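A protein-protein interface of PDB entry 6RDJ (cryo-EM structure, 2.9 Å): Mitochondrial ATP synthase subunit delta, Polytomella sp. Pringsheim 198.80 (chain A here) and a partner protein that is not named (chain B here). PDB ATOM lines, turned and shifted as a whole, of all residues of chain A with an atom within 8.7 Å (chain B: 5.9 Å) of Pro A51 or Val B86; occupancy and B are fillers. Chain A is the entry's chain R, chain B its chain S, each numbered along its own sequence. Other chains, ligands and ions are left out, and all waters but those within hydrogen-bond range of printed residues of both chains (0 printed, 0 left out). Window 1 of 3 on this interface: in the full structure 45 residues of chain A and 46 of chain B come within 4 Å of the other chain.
The backbone NH (N) of Val B207 sits at hydrogen-bond distance from the backbone carbonyl oxygen (O) of Glu A49 (3.0 Å). The side-chain carboxylate (OD1) of Asp B91 lies within hydrogen-bond range of the backbone NH (N) of Ser A52, 2.5 Å away. The side-chain hydroxyl of Thr A55 is in hydrogen-bond range of the side-chain carboxylate of Asp B83, at 3.3 Å. The backbone carbonyl oxygen (O) of Val A57 lies within hydrogen-bond range of the guanidinium group (NE) of Arg B87 (2.6 Å). NH1 of Arg B87 lies within salt-bridge range of OD2 of Asp A143 (3.4 Å). The backbone nitrogen (N) of Pro A51 sits close to the side-chain carboxylate (OD1) of Asp B91 (3.1 Å).
N of Phe A50 is in hydrogen-bond range of OD1 of Asn A53. O of Thr A55 is in hydrogen-bond range of NZ of Lys A58 (3.1 Å). The backbone carbonyl oxygen (O) of Phe A135 is in hydrogen-bond range of the backbone NH (N) of Asp A143 (2.8 Å). A ring nitrogen (ND1) of His A137 sits at hydrogen-bond distance from the side-chain carboxylate (OD2) of Asp A143, at 3.0 Å.
Among the printed residues, merely in contact across the chains: Glu A49 with Thr B206 (3.3 Å), Ala A59 with Arg B87 (3.3 Å), Pro A30 with Asp B91 (3.3 Å), Pro A51 with Val B207 (3.4 Å), Asp A143 with Pro B84 (3.5 Å), His A137 with Arg B87 (3.6 Å), Thr A55 with Arg B87 (3.6 Å), Phe A50 with Asp B91 (3.6 Å), Tyr A54 with Asp B83 (3.6 Å), Phe A50 with Val B207 (3.6 Å), Pro A51 with Val B86 (3.7 Å), Phe A135 with Leu B88 (3.7 Å), Thr A55 with Val B86 (3.7 Å), Pro A48 with Val B207 (3.8 Å), Ser A52 with Val B86 (3.8 Å), Phe A135 with Phe B85 (3.8 Å), His A137 with Leu B88 (3.9 Å), Pro A51 with Ala B208 (3.9 Å) and Phe A135 with Pro B84 (3.9 Å).
Pro A51 touches four residues of chain B. Val B86 touches three residues of chain A. No residue of chain A comes within 4 Å of Gly B90. Of the printed residues of chain B, Val A57 touches Arg B87 (2.6 Å). Of the printed residues of chain A, Val B207 touches Pro A48, Glu A49, Phe A50 and Pro A51. Of the printed residues of chain B, Pro A30 touches Asp B91. Of the printed residues of chain B, His A137 touches Arg B87 and Leu B88. Lys A58 touches none of the printed residues of chain B. The nearest residue of chain B that does not touch Pro A51 is Thr B206 (4.2 Å). The nearest printed residue of chain A that does not touch Thr B206 is Phe A50 (4.1 Å).
Of the 16 printed residues of chain A, 13 touch a printed residue of chain B. Hydrophobic or aromatic side chains of chain A that line the printed part of chain B: Pro A30, Pro A48, Phe A50, Pro A51, Val A57, Ala A59, Phe A135 and His A137. Of the 15 printed residues of chain B, 10 touch a printed residue of chain A. Among the printed residues, Asp or Glu carboxylates within 4 Å of a Lys or Arg side-chain nitrogen of the other chain: Asp A143 with Arg B87 (2.4 Å).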
ATOM      1  N   PRO A  30      18.280 -14.610  26.800  1.00  0.00           N
ATOM      2  CA  PRO A  30      18.082 -13.417  25.962  1.00  0.00           C
ATOM      3  C   PRO A  30      16.968 -13.566  24.942  1.00  0.00           C
ATOM      4  O   PRO A  30      16.213 -12.613  24.721  1.00  0.00           O
ATOM      5  CB  PRO A  30      19.450 -13.233  25.296  1.00  0.00           C
ATOM      6  CG  PRO A  30      20.099 -14.552  25.366  1.00  0.00           C
ATOM      7  CD  PRO A  30      19.608 -15.210  26.606  1.00  0.00           C
ATOM      8  N   PRO A  48      17.132  -4.215  24.532  1.00  0.00           N
ATOM      9  CA  PRO A  48      18.496  -3.962  24.992  1.00  0.00           C
ATOM     10  C   PRO A  48      19.415  -5.108  24.635  1.00  0.00           C
ATOM     11  O   PRO A  48      18.995  -6.257  24.498  1.00  0.00           O
ATOM     12  CB  PRO A  48      18.341  -3.823  26.510  1.00  0.00           C
ATOM     13  CG  PRO A  48      17.005  -4.375  26.819  1.00  0.00           C
ATOM     14  CD  PRO A  48      16.171  -4.071  25.633  1.00  0.00           C
ATOM     15  N   GLU A  49      20.685  -4.779  24.458  1.00  0.00           N
ATOM     16  CA  GLU A  49      21.664  -5.815  24.215  1.00  0.00           C
ATOM     17  C   GLU A  49      22.006  -6.519  25.520  1.00  0.00           C
ATOM     18  O   GLU A  49      21.659  -6.073  26.614  1.00  0.00           O
ATOM     19  CB  GLU A  49      22.910  -5.224  23.573  1.00  0.00           C
ATOM     20  CG  GLU A  49      22.596  -4.466  22.317  1.00  0.00           C
ATOM     21  CD  GLU A  49      22.360  -5.358  21.125  1.00  0.00           C
ATOM     22  OE1 GLU A  49      23.037  -6.398  21.008  1.00  0.00           O
ATOM     23  OE2 GLU A  49      21.489  -5.015  20.301  1.00  0.00           O
ATOM     24  N   PHE A  50      22.677  -7.651  25.393  1.00  0.00           N
ATOM     25  CA  PHE A  50      23.046  -8.481  26.523  1.00  0.00           C
ATOM     26  C   PHE A  50      24.505  -8.865  26.376  1.00  0.00           C
ATOM     27  O   PHE A  50      25.031  -8.875  25.260  1.00  0.00           O
ATOM     28  CB  PHE A  50      22.178  -9.744  26.585  1.00  0.00           C
ATOM     29  CG  PHE A  50      20.734  -9.491  26.327  1.00  0.00           C
ATOM     30  CD1 PHE A  50      20.185  -9.747  25.084  1.00  0.00           C
ATOM     31  CD2 PHE A  50      19.925  -8.988  27.322  1.00  0.00           C
ATOM     32  CE1 PHE A  50      18.855  -9.509  24.843  1.00  0.00           C
ATOM     33  CE2 PHE A  50      18.601  -8.749  27.086  1.00  0.00           C
ATOM     34  CZ  PHE A  50      18.064  -9.009  25.848  1.00  0.00           C
ATOM     35  N   PRO A  51      25.195  -9.174  27.479  1.00  0.00           N
ATOM     36  CA  PRO A  51      26.611  -9.553  27.365  1.00  0.00           C
ATOM     37  C   PRO A  51      26.862 -10.892  26.681  1.00  0.00           C
ATOM     38  O   PRO A  51      28.027 -11.207  26.414  1.00  0.00           O
ATOM     39  CB  PRO A  51      27.091  -9.574  28.822  1.00  0.00           C
ATOM     40  CG  PRO A  51      25.870  -9.483  29.662  1.00  0.00           C
ATOM     41  CD  PRO A  51      24.837  -8.804  28.857  1.00  0.00           C
ATOM     42  N   SER A  52      25.831 -11.682  26.375  1.00  0.00           N
ATOM     43  CA  SER A  52      26.046 -12.872  25.560  1.00  0.00           C
ATOM     44  C   SER A  52      26.259 -12.520  24.095  1.00  0.00           C
ATOM     45  O   SER A  52      26.922 -13.271  23.372  1.00  0.00           O
ATOM     46  CB  SER A  52      24.869 -13.828  25.693  1.00  0.00           C
ATOM     47  OG  SER A  52      23.645 -13.131  25.532  1.00  0.00           O
ATOM     48  N   ASN A  53      25.710 -11.395  23.637  1.00  0.00           N
ATOM     49  CA  ASN A  53      25.852 -11.020  22.237  1.00  0.00           C
ATOM     50  C   ASN A  53      27.224 -10.440  21.930  1.00  0.00           C
ATOM     51  O   ASN A  53      27.571 -10.294  20.756  1.00  0.00           O
ATOM     52  CB  ASN A  53      24.770 -10.016  21.847  1.00  0.00           C
ATOM     53  CG  ASN A  53      23.428 -10.336  22.468  1.00  0.00           C
ATOM     54  OD1 ASN A  53      22.806  -9.487  23.102  1.00  0.00           O
ATOM     55  ND2 ASN A  53      22.972 -11.568  22.286  1.00  0.00           N
ATOM     56  N   TYR A  54      28.010 -10.105  22.948  1.00  0.00           N
ATOM     57  CA  TYR A  54      29.345  -9.562  22.753  1.00  0.00           C
ATOM     58  C   TYR A  54      30.435 -10.571  23.068  1.00  0.00           C
ATOM     59  O   TYR A  54      31.616 -10.213  23.066  1.00  0.00           O
ATOM     60  CB  TYR A  54      29.533  -8.308  23.604  1.00  0.00           C
ATOM     61  CG  TYR A  54      28.539  -7.232  23.276  1.00  0.00           C
ATOM     62  CD1 TYR A  54      28.433  -6.745  21.985  1.00  0.00           C
ATOM     63  CD2 TYR A  54      27.702  -6.713  24.248  1.00  0.00           C
ATOM     64  CE1 TYR A  54      27.527  -5.770  21.672  1.00  0.00           C
ATOM     65  CE2 TYR A  54      26.792  -5.734  23.944  1.00  0.00           C
ATOM     66  CZ  TYR A  54      26.713  -5.268  22.655  1.00  0.00           C
ATOM     67  OH  TYR A  54      25.817  -4.290  22.332  1.00  0.00           O
ATOM     68  N   THR A  55      30.074 -11.816  23.336  1.00  0.00           N
ATOM     69  CA  THR A  55      31.049 -12.881  23.483  1.00  0.00           C
ATOM     70  C   THR A  55      30.912 -13.824  22.300  1.00  0.00           C
ATOM     71  O   THR A  55      29.866 -13.880  21.645  1.00  0.00           O
ATOM     72  CB  THR A  55      30.886 -13.634  24.819  1.00  0.00           C
ATOM     73  OG1 THR A  55      32.054 -14.422  25.070  1.00  0.00           O
ATOM     74  CG2 THR A  55      29.668 -14.538  24.806  1.00  0.00           C
ATOM     75  N   ALA A  56      31.994 -14.523  21.991  1.00  0.00           N
ATOM     76  CA  ALA A  56      32.008 -15.420  20.846  1.00  0.00           C
ATOM     77  C   ALA A  56      32.253 -16.861  21.249  1.00  0.00           C
ATOM     78  O   ALA A  56      31.490 -17.748  20.853  1.00  0.00           O
ATOM     79  CB  ALA A  56      33.069 -14.964  19.839  1.00  0.00           C
ATOM     80  N   VAL A  57      33.283 -17.116  22.046  1.00  0.00           N
ATOM     81  CA  VAL A  57      33.607 -18.473  22.463  1.00  0.00           C
ATOM     82  C   VAL A  57      32.685 -18.827  23.622  1.00  0.00           C
ATOM     83  O   VAL A  57      32.698 -18.161  24.658  1.00  0.00           O
ATOM     84  CB  VAL A  57      35.077 -18.599  22.874  1.00  0.00           C
ATOM     85  CG1 VAL A  57      35.402 -20.042  23.171  1.00  0.00           C
ATOM     86  CG2 VAL A  57      35.992 -18.023  21.811  1.00  0.00           C
ATOM     87  N   LYS A  58      31.881 -19.864  23.452  1.00  0.00           N
ATOM     88  CA  LYS A  58      31.013 -20.310  24.528  1.00  0.00           C
ATOM     89  C   LYS A  58      31.717 -21.418  25.309  1.00  0.00           C
ATOM     90  O   LYS A  58      32.915 -21.659  25.139  1.00  0.00           O
ATOM     91  CB  LYS A  58      29.660 -20.747  23.974  1.00  0.00           C
ATOM     92  CG  LYS A  58      28.591 -19.674  24.059  1.00  0.00           C
ATOM     93  CD  LYS A  58      28.852 -18.562  23.060  1.00  0.00           C
ATOM     94  CE  LYS A  58      27.834 -17.450  23.175  1.00  0.00           C
ATOM     95  NZ  LYS A  58      28.064 -16.415  22.132  1.00  0.00           N
ATOM     96  N   ALA A  59      30.986 -22.104  26.183  1.00  0.00           N
ATOM     97  CA  ALA A  59      31.574 -23.156  27.004  1.00  0.00           C
ATOM     98  C   ALA A  59      31.139 -24.552  26.579  1.00  0.00           C
ATOM     99  O   ALA A  59      31.979 -25.433  26.396  1.00  0.00           O
ATOM    100  CB  ALA A  59      31.223 -22.932  28.478  1.00  0.00           C
ATOM    101  N   PHE A 135      38.957 -20.759  35.081  1.00  0.00           N
ATOM    102  CA  PHE A 135      37.960 -21.709  34.629  1.00  0.00           C
ATOM    103  C   PHE A 135      38.495 -22.464  33.428  1.00  0.00           C
ATOM    104  O   PHE A 135      38.910 -21.853  32.443  1.00  0.00           O
ATOM    105  CB  PHE A 135      36.649 -21.021  34.259  1.00  0.00           C
ATOM    106  CG  PHE A 135      36.301 -19.865  35.135  1.00  0.00           C
ATOM    107  CD1 PHE A 135      36.155 -20.025  36.495  1.00  0.00           C
ATOM    108  CD2 PHE A 135      36.107 -18.617  34.592  1.00  0.00           C
ATOM    109  CE1 PHE A 135      35.839 -18.959  37.292  1.00  0.00           C
ATOM    110  CE2 PHE A 135      35.785 -17.552  35.386  1.00  0.00           C
ATOM    111  CZ  PHE A 135      35.651 -17.724  36.736  1.00  0.00           C
ATOM    112  N   HIS A 137      36.904 -24.802  30.758  1.00  0.00           N
ATOM    113  CA  HIS A 137      35.547 -25.037  30.315  1.00  0.00           C
ATOM    114  C   HIS A 137      35.461 -26.394  29.636  1.00  0.00           C
ATOM    115  O   HIS A 137      36.494 -27.016  29.380  1.00  0.00           O
ATOM    116  CB  HIS A 137      35.122 -23.898  29.391  1.00  0.00           C
ATOM    117  CG  HIS A 137      34.828 -22.634  30.130  1.00  0.00           C
ATOM    118  ND1 HIS A 137      35.712 -21.580  30.181  1.00  0.00           N
ATOM    119  CD2 HIS A 137      33.774 -22.275  30.895  1.00  0.00           C
ATOM    120  CE1 HIS A 137      35.201 -20.618  30.926  1.00  0.00           C
ATOM    121  NE2 HIS A 137      34.025 -21.015  31.371  1.00  0.00           N
ATOM    122  N   ASP A 143      40.264 -19.827  31.082  1.00  0.00           N
ATOM    123  CA  ASP A 143      39.956 -18.428  31.347  1.00  0.00           C
ATOM    124  C   ASP A 143      40.538 -18.040  32.695  1.00  0.00           C
ATOM    125  O   ASP A 143      39.854 -18.118  33.714  1.00  0.00           O
ATOM    126  CB  ASP A 143      38.479 -18.215  31.328  1.00  0.00           C
ATOM    127  CG  ASP A 143      37.903 -18.330  29.954  1.00  0.00           C
ATOM    128  OD1 ASP A 143      37.694 -17.290  29.303  1.00  0.00           O
ATOM    129  OD2 ASP A 143      37.673 -19.467  29.510  1.00  0.00           O
ATOM    130  N   VAL B  82      34.743  -9.806  30.973  1.00  0.00           N
ATOM    131  CA  VAL B  82      33.308 -10.037  31.035  1.00  0.00           C
ATOM    132  C   VAL B  82      32.952 -11.385  30.426  1.00  0.00           C
ATOM    133  O   VAL B  82      32.036 -12.063  30.901  1.00  0.00           O
ATOM    134  CB  VAL B  82      32.579  -8.876  30.338  1.00  0.00           C
ATOM    135  CG1 VAL B  82      31.092  -8.979  30.525  1.00  0.00           C
ATOM    136  CG2 VAL B  82      33.073  -7.580  30.878  1.00  0.00           C
ATOM    137  N   ASP B  83      33.685 -11.815  29.403  1.00  0.00           N
ATOM    138  CA  ASP B  83      33.392 -13.044  28.666  1.00  0.00           C
ATOM    139  C   ASP B  83      33.487 -14.370  29.435  1.00  0.00           C
ATOM    140  O   ASP B  83      32.638 -15.239  29.187  1.00  0.00           O
ATOM    141  CB  ASP B  83      34.272 -13.119  27.415  1.00  0.00           C
ATOM    142  CG  ASP B  83      34.265 -11.835  26.620  1.00  0.00           C
ATOM    143  OD1 ASP B  83      35.315 -11.168  26.554  1.00  0.00           O
ATOM    144  OD2 ASP B  83      33.200 -11.481  26.068  1.00  0.00           O
ATOM    145  N   PRO B  84      34.460 -14.605  30.336  1.00  0.00           N
ATOM    146  CA  PRO B  84      34.437 -15.876  31.082  1.00  0.00           C
ATOM    147  C   PRO B  84      33.252 -16.034  32.004  1.00  0.00           C
ATOM    148  O   PRO B  84      32.746 -17.150  32.149  1.00  0.00           O
ATOM    149  CB  PRO B  84      35.744 -15.840  31.877  1.00  0.00           C
ATOM    150  CG  PRO B  84      36.123 -14.468  31.894  1.00  0.00           C
ATOM    151  CD  PRO B  84      35.752 -13.947  30.584  1.00  0.00           C
ATOM    152  N   PHE B  85      32.773 -14.959  32.610  1.00  0.00           N
ATOM    153  CA  PHE B  85      31.603 -15.075  33.457  1.00  0.00           C
ATOM    154  C   PHE B  85      30.322 -15.197  32.666  1.00  0.00           C
ATOM    155  O   PHE B  85      29.339 -15.725  33.190  1.00  0.00           O
ATOM    156  CB  PHE B  85      31.495 -13.876  34.375  1.00  0.00           C
ATOM    157  CG  PHE B  85      32.598 -13.771  35.342  1.00  0.00           C
ATOM    158  CD1 PHE B  85      32.633 -14.589  36.444  1.00  0.00           C
ATOM    159  CD2 PHE B  85      33.607 -12.856  35.154  1.00  0.00           C
ATOM    160  CE1 PHE B  85      33.650 -14.495  37.335  1.00  0.00           C
ATOM    161  CE2 PHE B  85      34.625 -12.763  36.044  1.00  0.00           C
ATOM    162  CZ  PHE B  85      34.645 -13.589  37.130  1.00  0.00           C
ATOM    163  N   VAL B  86      30.293 -14.704  31.435  1.00  0.00           N
ATOM    164  CA  VAL B  86      29.077 -14.828  30.650  1.00  0.00           C
ATOM    165  C   VAL B  86      29.062 -16.152  29.899  1.00  0.00           C
ATOM    166  O   VAL B  86      28.003 -16.571  29.415  1.00  0.00           O
ATOM    167  CB  VAL B  86      28.911 -13.628  29.699  1.00  0.00           C
ATOM    168  CG1 VAL B  86      29.748 -13.791  28.459  1.00  0.00           C
ATOM    169  CG2 VAL B  86      27.450 -13.380  29.367  1.00  0.00           C
ATOM    170  N   ARG B  87      30.200 -16.840  29.804  1.00  0.00           N
ATOM    171  CA  ARG B  87      30.185 -18.199  29.291  1.00  0.00           C
ATOM    172  C   ARG B  87      30.148 -19.243  30.394  1.00  0.00           C
ATOM    173  O   ARG B  87      29.807 -20.396  30.120  1.00  0.00           O
ATOM    174  CB  ARG B  87      31.389 -18.448  28.382  1.00  0.00           C
ATOM    175  CG  ARG B  87      32.699 -18.601  29.096  1.00  0.00           C
ATOM    176  CD  ARG B  87      33.770 -18.994  28.112  1.00  0.00           C
ATOM    177  NE  ARG B  87      33.876 -18.035  27.023  1.00  0.00           N
ATOM    178  CZ  ARG B  87      34.909 -17.225  26.847  1.00  0.00           C
ATOM    179  NH1 ARG B  87      35.930 -17.257  27.683  1.00  0.00           N
ATOM    180  NH2 ARG B  87      34.926 -16.384  25.831  1.00  0.00           N
ATOM    181  N   LEU B  88      30.467 -18.867  31.628  1.00  0.00           N
ATOM    182  CA  LEU B  88      30.395 -19.779  32.759  1.00  0.00           C
ATOM    183  C   LEU B  88      29.027 -19.763  33.420  1.00  0.00           C
ATOM    184  O   LEU B  88      28.494 -20.819  33.767  1.00  0.00           O
ATOM    185  CB  LEU B  88      31.467 -19.412  33.785  1.00  0.00           C
ATOM    186  CG  LEU B  88      31.536 -20.221  35.076  1.00  0.00           C
ATOM    187  CD1 LEU B  88      32.130 -21.579  34.814  1.00  0.00           C
ATOM    188  CD2 LEU B  88      32.342 -19.480  36.109  1.00  0.00           C
ATOM    189  N   PHE B  89      28.450 -18.582  33.603  1.00  0.00           N
ATOM    190  CA  PHE B  89      27.149 -18.423  34.231  1.00  0.00           C
ATOM    191  C   PHE B  89      26.039 -18.156  33.233  1.00  0.00           C
ATOM    192  O   PHE B  89      24.885 -18.026  33.642  1.00  0.00           O
ATOM    193  CB  PHE B  89      27.181 -17.278  35.237  1.00  0.00           C
ATOM    194  CG  PHE B  89      28.014 -17.548  36.435  1.00  0.00           C
ATOM    195  CD1 PHE B  89      28.204 -18.836  36.886  1.00  0.00           C
ATOM    196  CD2 PHE B  89      28.601 -16.509  37.125  1.00  0.00           C
ATOM    197  CE1 PHE B  89      28.967 -19.079  37.995  1.00  0.00           C
ATOM    198  CE2 PHE B  89      29.365 -16.750  38.231  1.00  0.00           C
ATOM    199  CZ  PHE B  89      29.545 -18.032  38.667  1.00  0.00           C
ATOM    200  N   GLY B  90      26.357 -18.034  31.952  1.00  0.00           N
ATOM    201  CA  GLY B  90      25.329 -17.740  30.981  1.00  0.00           C
ATOM    202  C   GLY B  90      24.876 -16.290  31.052  1.00  0.00           C
ATOM    203  O   GLY B  90      25.549 -15.416  31.595  1.00  0.00           O
ATOM    204  N   ASP B  91      23.687 -16.053  30.502  1.00  0.00           N
ATOM    205  CA  ASP B  91      23.127 -14.707  30.412  1.00  0.00           C
ATOM    206  C   ASP B  91      21.622 -14.833  30.614  1.00  0.00           C
ATOM    207  O   ASP B  91      20.910 -15.218  29.685  1.00  0.00           O
ATOM    208  CB  ASP B  91      23.448 -14.083  29.065  1.00  0.00           C
ATOM    209  CG  ASP B  91      23.541 -12.585  29.124  1.00  0.00           C
ATOM    210  OD1 ASP B  91      24.312 -12.022  28.326  1.00  0.00           O
ATOM    211  OD2 ASP B  91      22.861 -11.970  29.973  1.00  0.00           O
ATOM    212  N   THR B 206      22.407  -1.666  27.294  1.00  0.00           N
ATOM    213  CA  THR B 206      22.695  -3.054  27.599  1.00  0.00           C
ATOM    214  C   THR B 206      22.216  -3.344  29.006  1.00  0.00           C
ATOM    215  O   THR B 206      22.384  -2.520  29.906  1.00  0.00           O
ATOM    216  CB  THR B 206      24.196  -3.329  27.461  1.00  0.00           C
ATOM    217  OG1 THR B 206      24.604  -2.990  26.134  1.00  0.00           O
ATOM    218  CG2 THR B 206      24.534  -4.782  27.704  1.00  0.00           C
ATOM    219  N   VAL B 207      21.580  -4.493  29.185  1.00  0.00           N
ATOM    220  CA  VAL B 207      21.222  -4.989  30.502  1.00  0.00           C
ATOM    221  C   VAL B 207      22.057  -6.231  30.791  1.00  0.00           C
ATOM    222  O   VAL B 207      22.065  -7.190  30.012  1.00  0.00           O
ATOM    223  CB  VAL B 207      19.707  -5.231  30.625  1.00  0.00           C
ATOM    224  CG1 VAL B 207      19.161  -6.040  29.467  1.00  0.00           C
ATOM    225  CG2 VAL B 207      19.399  -5.903  31.935  1.00  0.00           C
ATOM    226  N   ALA B 208      22.820  -6.176  31.874  1.00  0.00           N
ATOM    227  CA  ALA B 208      23.732  -7.242  32.251  1.00  0.00           C
ATOM    228  C   ALA B 208      23.294  -7.764  33.604  1.00  0.00           C
ATOM    229  O   ALA B 208      23.234  -7.002  34.571  1.00  0.00           O
ATOM    230  CB  ALA B 208      25.168  -6.739  32.301  1.00  0.00           C
ATOM    231  N   THR B 209      22.992  -9.052  33.671  1.00  0.00           N
ATOM    232  CA  THR B 209      22.359  -9.640  34.838  1.00  0.00           C
ATOM    233  C   THR B 209      23.343 -10.524  35.587  1.00  0.00           C
ATOM    234  O   THR B 209      24.055 -11.323  34.976  1.00  0.00           O
ATOM    235  CB  THR B 209      21.123 -10.430  34.428  1.00  0.00           C
ATOM    236  OG1 THR B 209      20.322  -9.605  33.582  1.00  0.00           O
ATOM    237  CG2 THR B 209      20.305 -10.789  35.640  1.00  0.00           C
ATOM    238  N   HIS B 250      32.036 -11.321  39.708  1.00  0.00           N
ATOM    239  CA  HIS B 250      31.315 -11.086  38.463  1.00  0.00           C
ATOM    240  C   HIS B 250      30.583  -9.755  38.488  1.00  0.00           C
ATOM    241  O   HIS B 250      30.525  -9.060  37.470  1.00  0.00           O
ATOM    242  CB  HIS B 250      30.354 -12.242  38.223  1.00  0.00           C
ATOM    243  CG  HIS B 250      29.466 -12.075  37.036  1.00  0.00           C
ATOM    244  ND1 HIS B 250      29.872 -11.448  35.882  1.00  0.00           N
ATOM    245  CD2 HIS B 250      28.220 -12.538  36.791  1.00  0.00           C
ATOM    246  CE1 HIS B 250      28.902 -11.497  34.991  1.00  0.00           C
ATOM    247  NE2 HIS B 250      27.887 -12.155  35.518  1.00  0.00           N
